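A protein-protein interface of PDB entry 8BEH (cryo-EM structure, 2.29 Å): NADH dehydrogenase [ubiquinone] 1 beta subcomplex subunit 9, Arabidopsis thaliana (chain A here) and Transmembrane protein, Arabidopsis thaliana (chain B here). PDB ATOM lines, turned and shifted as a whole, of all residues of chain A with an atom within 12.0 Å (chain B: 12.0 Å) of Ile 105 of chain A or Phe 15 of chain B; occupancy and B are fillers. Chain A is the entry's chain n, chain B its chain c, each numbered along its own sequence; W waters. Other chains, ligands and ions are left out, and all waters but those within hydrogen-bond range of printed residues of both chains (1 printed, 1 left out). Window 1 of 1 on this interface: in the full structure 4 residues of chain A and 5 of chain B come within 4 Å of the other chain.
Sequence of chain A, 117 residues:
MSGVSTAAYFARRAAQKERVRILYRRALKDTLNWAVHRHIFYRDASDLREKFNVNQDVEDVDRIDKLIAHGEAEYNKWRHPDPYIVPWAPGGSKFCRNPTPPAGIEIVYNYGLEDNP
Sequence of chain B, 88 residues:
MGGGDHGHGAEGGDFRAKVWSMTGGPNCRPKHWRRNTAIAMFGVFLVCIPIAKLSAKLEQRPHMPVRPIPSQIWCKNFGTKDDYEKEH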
ATOM      1  N   ASN A  98      23.651 -10.449  12.956  1.00  0.00           N
ATOM      2  CA  ASN A  98      23.543 -11.928  12.866  1.00  0.00           C
ATOM      3  C   ASN A  98      24.636 -12.533  11.955  1.00  0.00           C
ATOM      4  O   ASN A  98      24.308 -13.266  11.090  1.00  0.00           O
ATOM      5  CB  ASN A  98      22.100 -12.344  12.597  1.00  0.00           C
ATOM      6  CG  ASN A  98      21.121 -11.776  13.596  1.00  0.00           C
ATOM      7  OD1 ASN A  98      21.408 -11.720  14.782  1.00  0.00           O
ATOM      8  ND2 ASN A  98      19.971 -11.345  13.123  1.00  0.00           N
ATOM      9  N   PRO A  99      25.922 -12.241  12.170  1.00  0.00           N
ATOM     10  CA  PRO A  99      26.965 -12.865  11.353  1.00  0.00           C
ATOM     11  C   PRO A  99      27.041 -14.362  11.582  1.00  0.00           C
ATOM     12  O   PRO A  99      26.672 -14.875  12.640  1.00  0.00           O
ATOM     13  CB  PRO A  99      28.242 -12.170  11.829  1.00  0.00           C
ATOM     14  CG  PRO A  99      27.952 -11.814  13.248  1.00  0.00           C
ATOM     15  CD  PRO A  99      26.482 -11.506  13.318  1.00  0.00           C
ATOM     16  N   THR A 100      27.519 -15.059  10.565  1.00  0.00           N
ATOM     17  CA  THR A 100      27.837 -16.463  10.742  1.00  0.00           C
ATOM     18  C   THR A 100      28.971 -16.595  11.755  1.00  0.00           C
ATOM     19  O   THR A 100      29.892 -15.771  11.766  1.00  0.00           O
ATOM     20  CB  THR A 100      28.231 -17.109   9.411  1.00  0.00           C
ATOM     21  OG1 THR A 100      27.135 -17.018   8.494  1.00  0.00           O
ATOM     22  CG2 THR A 100      28.592 -18.561   9.608  1.00  0.00           C
ATOM     23  N   PRO A 101      28.920 -17.591  12.634  1.00  0.00           N
ATOM     24  CA  PRO A 101      29.961 -17.721  13.644  1.00  0.00           C
ATOM     25  C   PRO A 101      31.297 -18.029  13.003  1.00  0.00           C
ATOM     26  O   PRO A 101      31.363 -18.662  11.932  1.00  0.00           O
ATOM     27  CB  PRO A 101      29.471 -18.889  14.511  1.00  0.00           C
ATOM     28  CG  PRO A 101      28.055 -19.094  14.161  1.00  0.00           C
ATOM     29  CD  PRO A 101      27.862 -18.604  12.773  1.00  0.00           C
ATOM     30  N   PRO A 102      32.392 -17.597  13.618  1.00  0.00           N
ATOM     31  CA  PRO A 102      33.715 -17.983  13.119  1.00  0.00           C
ATOM     32  C   PRO A 102      33.941 -19.478  13.263  1.00  0.00           C
ATOM     33  O   PRO A 102      33.378 -20.137  14.141  1.00  0.00           O
ATOM     34  CB  PRO A 102      34.684 -17.191  14.003  1.00  0.00           C
ATOM     35  CG  PRO A 102      33.906 -16.827  15.220  1.00  0.00           C
ATOM     36  CD  PRO A 102      32.453 -16.800  14.855  1.00  0.00           C
ATOM     37  N   ALA A 103      34.766 -20.014  12.372  1.00  0.00           N
ATOM     38  CA  ALA A 103      35.206 -21.392  12.487  1.00  0.00           C
ATOM     39  C   ALA A 103      36.420 -21.485  13.407  1.00  0.00           C
ATOM     40  O   ALA A 103      37.131 -20.505  13.644  1.00  0.00           O
ATOM     41  CB  ALA A 103      35.541 -21.970  11.115  1.00  0.00           C
ATOM     42  N   GLY A 104      36.653 -22.685  13.926  1.00  0.00           N
ATOM     43  CA  GLY A 104      37.773 -22.920  14.813  1.00  0.00           C
ATOM     44  C   GLY A 104      37.501 -22.702  16.281  1.00  0.00           C
ATOM     45  O   GLY A 104      38.452 -22.561  17.057  1.00  0.00           O
ATOM     46  N   ILE A 105      36.239 -22.671  16.693  1.00  0.00           N
ATOM     47  CA  ILE A 105      35.867 -22.438  18.081  1.00  0.00           C
ATOM     48  C   ILE A 105      35.562 -23.781  18.718  1.00  0.00           C
ATOM     49  O   ILE A 105      34.754 -24.554  18.195  1.00  0.00           O
ATOM     50  CB  ILE A 105      34.656 -21.493  18.184  1.00  0.00           C
ATOM     51  CG1 ILE A 105      34.998 -20.112  17.619  1.00  0.00           C
ATOM     52  CG2 ILE A 105      34.180 -21.388  19.627  1.00  0.00           C
ATOM     53  CD1 ILE A 105      36.319 -19.550  18.089  1.00  0.00           C
ATOM     54  N   GLU A 106      36.261 -24.059  19.809  1.00  0.00           N
ATOM     55  CA  GLU A 106      36.064 -25.298  20.590  1.00  0.00           C
ATOM     56  C   GLU A 106      35.451 -24.986  21.972  1.00  0.00           C
ATOM     57  O   GLU A 106      35.859 -24.011  22.574  1.00  0.00           O
ATOM     58  CB  GLU A 106      37.401 -26.021  20.641  1.00  0.00           C
ATOM     59  CG  GLU A 106      37.951 -26.344  19.280  1.00  0.00           C
ATOM     60  CD  GLU A 106      39.455 -26.485  19.204  1.00  0.00           C
ATOM     61  OE1 GLU A 106      40.018 -27.155  20.068  1.00  0.00           O
ATOM     62  OE2 GLU A 106      40.052 -25.935  18.255  1.00  0.00           O
ATOM     63  N   ILE A 107      34.493 -25.750  22.435  1.00  0.00           N
ATOM     64  CA  ILE A 107      33.900 -25.586  23.754  1.00  0.00           C
ATOM     65  C   ILE A 107      34.369 -26.745  24.618  1.00  0.00           C
ATOM     66  O   ILE A 107      34.251 -27.909  24.217  1.00  0.00           O
ATOM     67  CB  ILE A 107      32.362 -25.547  23.674  1.00  0.00           C
ATOM     68  CG1 ILE A 107      31.882 -24.377  22.806  1.00  0.00           C
ATOM     69  CG2 ILE A 107      31.754 -25.467  25.060  1.00  0.00           C
ATOM     70  CD1 ILE A 107      32.410 -23.025  23.205  1.00  0.00           C
ATOM     71  N   VAL A 108      34.901 -26.467  25.782  1.00  0.00           N
ATOM     72  CA  VAL A 108      35.483 -27.532  26.655  1.00  0.00           C
ATOM     73  C   VAL A 108      34.477 -27.861  27.746  1.00  0.00           C
ATOM     74  O   VAL A 108      33.851 -26.964  28.313  1.00  0.00           O
ATOM     75  CB  VAL A 108      36.860 -27.166  27.277  1.00  0.00           C
ATOM     76  CG1 VAL A 108      37.522 -28.262  28.075  1.00  0.00           C
ATOM     77  CG2 VAL A 108      37.806 -26.470  26.338  1.00  0.00           C
ATOM     78  N   TYR A 109      34.389 -29.109  28.048  1.00  0.00           N
ATOM     79  CA  TYR A 109      33.522 -29.654  29.077  1.00  0.00           C
ATOM     80  C   TYR A 109      34.367 -30.154  30.241  1.00  0.00           C
ATOM     81  O   TYR A 109      35.546 -30.479  30.075  1.00  0.00           O
ATOM     82  CB  TYR A 109      32.670 -30.796  28.517  1.00  0.00           C
ATOM     83  CG  TYR A 109      31.578 -30.339  27.584  1.00  0.00           C
ATOM     84  CD1 TYR A 109      31.026 -29.071  27.695  1.00  0.00           C
ATOM     85  CD2 TYR A 109      31.132 -31.161  26.561  1.00  0.00           C
ATOM     86  CE1 TYR A 109      30.033 -28.651  26.835  1.00  0.00           C
ATOM     87  CE2 TYR A 109      30.149 -30.752  25.697  1.00  0.00           C
ATOM     88  CZ  TYR A 109      29.602 -29.496  25.835  1.00  0.00           C
ATOM     89  OH  TYR A 109      28.618 -29.091  24.969  1.00  0.00           O
ATOM     90  N   GLY B  13      25.291 -21.692  15.333  1.00  0.00           N
ATOM     91  CA  GLY B  13      26.068 -22.085  14.174  1.00  0.00           C
ATOM     92  C   GLY B  13      26.535 -23.519  14.265  1.00  0.00           C
ATOM     93  O   GLY B  13      25.740 -24.451  14.152  1.00  0.00           O
ATOM     94  N   ASP B  14      27.836 -23.700  14.468  1.00  0.00           N
ATOM     95  CA  ASP B  14      28.400 -25.021  14.701  1.00  0.00           C
ATOM     96  C   ASP B  14      28.824 -25.216  16.151  1.00  0.00           C
ATOM     97  O   ASP B  14      28.437 -26.206  16.778  1.00  0.00           O
ATOM     98  CB  ASP B  14      29.586 -25.264  13.762  1.00  0.00           C
ATOM     99  CG  ASP B  14      29.157 -25.810  12.415  1.00  0.00           C
ATOM    100  OD1 ASP B  14      29.012 -25.014  11.463  1.00  0.00           O
ATOM    101  OD2 ASP B  14      28.968 -27.040  12.306  1.00  0.00           O
ATOM    102  N   PHE B  15      29.600 -24.288  16.707  1.00  0.00           N
ATOM    103  CA  PHE B  15      29.992 -24.412  18.103  1.00  0.00           C
ATOM    104  C   PHE B  15      28.866 -24.046  19.064  1.00  0.00           C
ATOM    105  O   PHE B  15      28.854 -24.538  20.194  1.00  0.00           O
ATOM    106  CB  PHE B  15      31.243 -23.565  18.385  1.00  0.00           C
ATOM    107  CG  PHE B  15      30.988 -22.086  18.483  1.00  0.00           C
ATOM    108  CD1 PHE B  15      30.577 -21.509  19.678  1.00  0.00           C
ATOM    109  CD2 PHE B  15      31.203 -21.264  17.393  1.00  0.00           C
ATOM    110  CE1 PHE B  15      30.351 -20.155  19.766  1.00  0.00           C
ATOM    111  CE2 PHE B  15      30.987 -19.909  17.479  1.00  0.00           C
ATOM    112  CZ  PHE B  15      30.557 -19.352  18.668  1.00  0.00           C
ATOM    113  N   ARG B  16      27.923 -23.202  18.642  1.00  0.00           N
ATOM    114  CA  ARG B  16      26.873 -22.742  19.542  1.00  0.00           C
ATOM    115  C   ARG B  16      25.922 -23.862  19.957  1.00  0.00           C
ATOM    116  O   ARG B  16      25.232 -23.729  20.971  1.00  0.00           O
ATOM    117  CB  ARG B  16      26.106 -21.590  18.890  1.00  0.00           C
ATOM    118  CG  ARG B  16      26.895 -20.275  18.862  1.00  0.00           C
ATOM    119  CD  ARG B  16      26.084 -19.125  18.283  1.00  0.00           C
ATOM    120  NE  ARG B  16      25.720 -19.357  16.894  1.00  0.00           N
ATOM    121  CZ  ARG B  16      25.199 -18.443  16.085  1.00  0.00           C
ATOM    122  NH1 ARG B  16      24.966 -17.209  16.495  1.00  0.00           N
ATOM    123  NH2 ARG B  16      24.903 -18.778  14.834  1.00  0.00           N
ATOM    124  N   ALA B  17      25.883 -24.965  19.208  1.00  0.00           N
ATOM    125  CA  ALA B  17      25.108 -26.131  19.610  1.00  0.00           C
ATOM    126  C   ALA B  17      25.674 -26.812  20.847  1.00  0.00           C
ATOM    127  O   ALA B  17      24.987 -27.641  21.447  1.00  0.00           O
ATOM    128  CB  ALA B  17      25.039 -27.136  18.462  1.00  0.00           C
ATOM    129  N   LYS B  18      26.902 -26.492  21.239  1.00  0.00           N
ATOM    130  CA  LYS B  18      27.493 -27.030  22.450  1.00  0.00           C
ATOM    131  C   LYS B  18      27.475 -26.033  23.597  1.00  0.00           C
ATOM    132  O   LYS B  18      28.100 -26.284  24.631  1.00  0.00           O
ATOM    133  CB  LYS B  18      28.924 -27.490  22.173  1.00  0.00           C
ATOM    134  CG  LYS B  18      29.064 -28.300  20.902  1.00  0.00           C
ATOM    135  CD  LYS B  18      30.509 -28.395  20.469  1.00  0.00           C
ATOM    136  CE  LYS B  18      31.227 -29.517  21.194  1.00  0.00           C
ATOM    137  NZ  LYS B  18      31.830 -29.076  22.472  1.00  0.00           N
ATOM    138  N   VAL B  19      26.776 -24.915  23.446  1.00  0.00           N
ATOM    139  CA  VAL B  19      26.798 -23.837  24.425  1.00  0.00           C
ATOM    140  C   VAL B  19      25.427 -23.770  25.085  1.00  0.00           C
ATOM    141  O   VAL B  19      24.415 -23.543  24.414  1.00  0.00           O
ATOM    142  CB  VAL B  19      27.174 -22.495  23.780  1.00  0.00           C
ATOM    143  CG1 VAL B  19      26.825 -21.337  24.706  1.00  0.00           C
ATOM    144  CG2 VAL B  19      28.648 -22.478  23.390  1.00  0.00           C
ATOM    145  N   TRP B  20      25.400 -23.956  26.399  1.00  0.00           N
ATOM    146  CA  TRP B  20      24.172 -23.936  27.179  1.00  0.00           C
ATOM    147  C   TRP B  20      23.859 -22.506  27.605  1.00  0.00           C
ATOM    148  O   TRP B  20      24.744 -21.790  28.076  1.00  0.00           O
ATOM    149  CB  TRP B  20      24.324 -24.845  28.401  1.00  0.00           C
ATOM    150  CG  TRP B  20      23.060 -25.116  29.169  1.00  0.00           C
ATOM    151  CD1 TRP B  20      22.296 -26.241  29.108  1.00  0.00           C
ATOM    152  CD2 TRP B  20      22.435 -24.259  30.131  1.00  0.00           C
ATOM    153  NE1 TRP B  20      21.229 -26.136  29.959  1.00  0.00           N
ATOM    154  CE2 TRP B  20      21.289 -24.929  30.601  1.00  0.00           C
ATOM    155  CE3 TRP B  20      22.726 -22.987  30.636  1.00  0.00           C
ATOM    156  CZ2 TRP B  20      20.435 -24.372  31.551  1.00  0.00           C
ATOM    157  CZ3 TRP B  20      21.882 -22.439  31.580  1.00  0.00           C
ATOM    158  CH2 TRP B  20      20.748 -23.129  32.026  1.00  0.00           C
ATOM    159  N   SER B  21      22.608 -22.085  27.417  1.00  0.00           N
ATOM    160  CA  SER B  21      22.134 -20.811  27.941  1.00  0.00           C
ATOM    161  C   SER B  21      20.725 -20.981  28.495  1.00  0.00           C
ATOM    162  O   SER B  21      20.005 -21.916  28.142  1.00  0.00           O
ATOM    163  CB  SER B  21      22.147 -19.692  26.886  1.00  0.00           C
ATOM    164  OG  SER B  21      21.440 -20.057  25.721  1.00  0.00           O
ATOM    165  N   GLY B  24      18.177 -20.172  25.715  1.00  0.00           N
ATOM    166  CA  GLY B  24      18.109 -21.206  24.709  1.00  0.00           C
ATOM    167  C   GLY B  24      19.028 -21.040  23.518  1.00  0.00           C
ATOM    168  O   GLY B  24      19.139 -21.975  22.722  1.00  0.00           O
ATOM    169  N   GLY B  25      19.679 -19.895  23.359  1.00  0.00           N
ATOM    170  CA  GLY B  25      20.576 -19.691  22.245  1.00  0.00           C
ATOM    171  C   GLY B  25      19.854 -19.479  20.926  1.00  0.00           C
ATOM    172  O   GLY B  25      18.640 -19.276  20.885  1.00  0.00           O
ATOM    173  N   PRO B  26      20.592 -19.537  19.820  1.00  0.00           N
ATOM    174  CA  PRO B  26      20.009 -19.192  18.517  1.00  0.00           C
ATOM    175  C   PRO B  26      19.110 -20.281  17.947  1.00  0.00           C
ATOM    176  O   PRO B  26      19.445 -21.467  17.968  1.00  0.00           O
ATOM    177  CB  PRO B  26      21.244 -18.983  17.632  1.00  0.00           C
ATOM    178  CG  PRO B  26      22.284 -19.854  18.246  1.00  0.00           C
ATOM    179  CD  PRO B  26      22.027 -19.856  19.722  1.00  0.00           C
ATOM    180  N   ASN B  27      17.964 -19.849  17.413  1.00  0.00           N
ATOM    181  CA  ASN B  27      17.025 -20.722  16.701  1.00  0.00           C
ATOM    182  C   ASN B  27      16.561 -21.884  17.579  1.00  0.00           C
ATOM    183  O   ASN B  27      16.600 -23.046  17.181  1.00  0.00           O
ATOM    184  CB  ASN B  27      17.639 -21.234  15.396  1.00  0.00           C
ATOM    185  CG  ASN B  27      17.952 -20.120  14.421  1.00  0.00           C
ATOM    186  OD1 ASN B  27      17.077 -19.347  14.044  1.00  0.00           O
ATOM    187  ND2 ASN B  27      19.212 -20.015  14.029  1.00  0.00           N
HETATM  188  O   HOH W   1      34.246 -27.971  20.789  1.00  0.00           O
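Water W1 bridges N of Ile 107 of chain A (2.8 Å) and NZ of Lys 18 of chain B (3.1 Å).
Printed residues of chain B that touch a printed residue of chain A: Gly 13, Phe 15, Arg 16, Lys 18 and Val 19.
Hydrophobic or aromatic side chains of chain A that line the printed part of chain B: Pro 101, Ile 105, Ile 107 and Tyr 109.
Along chain A the printed residues that touch a printed residue of chain B span positions 101 to 109.
Gly 13 of chain B touches Pro 101 of chain A.
Pro 101 of chain A touches Phe 15 of chain B.
Pro 101 of chain A touches Arg 16 of chain B (CG to NH2, 3.2 Å).
Phe 15 of chain B touches Ile 105 of chain A.
Val 19 of chain B touches Ile 107 of chain A (CG2 to CG1, 3.8 Å).
The backbone carbonyl oxygen (O) of Ile 107 of chain A lies within hydrogen-bond range of the side-chain amino group (NZ) of Lys 18 of chain B.
The side-chain hydroxyl (OH) of Tyr 109 of chain A lies within hydrogen-bond range of the backbone carbonyl oxygen (O) of Lys 18 of chain B, 2.9 Å away.
Of chain B, only Gly 13, Phe 15 and Arg 16 come within 4 Å of Pro 101 of chain A.
No residue of chain B comes within 4 Å of Pro 102 of chain A.
No residue of chain B comes within 4 Å of Ala 103 of chain A.
Ile 105 of chain A touches just one residue of chain B: Phe 15.
No residue of chain B comes within 4 Å of Glu 106 of chain A.
Of the printed residues of chain B, Ile 107 of chain A touches Lys 18 (3.2 Å) and Val 19 (3.8 Å).
Printed residues of chain B within 4 Å of Tyr 109 of chain A: Lys 18.
Of chain A, only Pro 101 comes within 4 Å of Gly 13 of chain B.
No residue of chain A comes within 4 Å of Asp 14 of chain B.
Printed residues of chain A within 4 Å of Phe 15 of chain B: Pro 101 and Ile 105.
Arg 16 of chain B touches just one residue of chain A: Pro 101.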
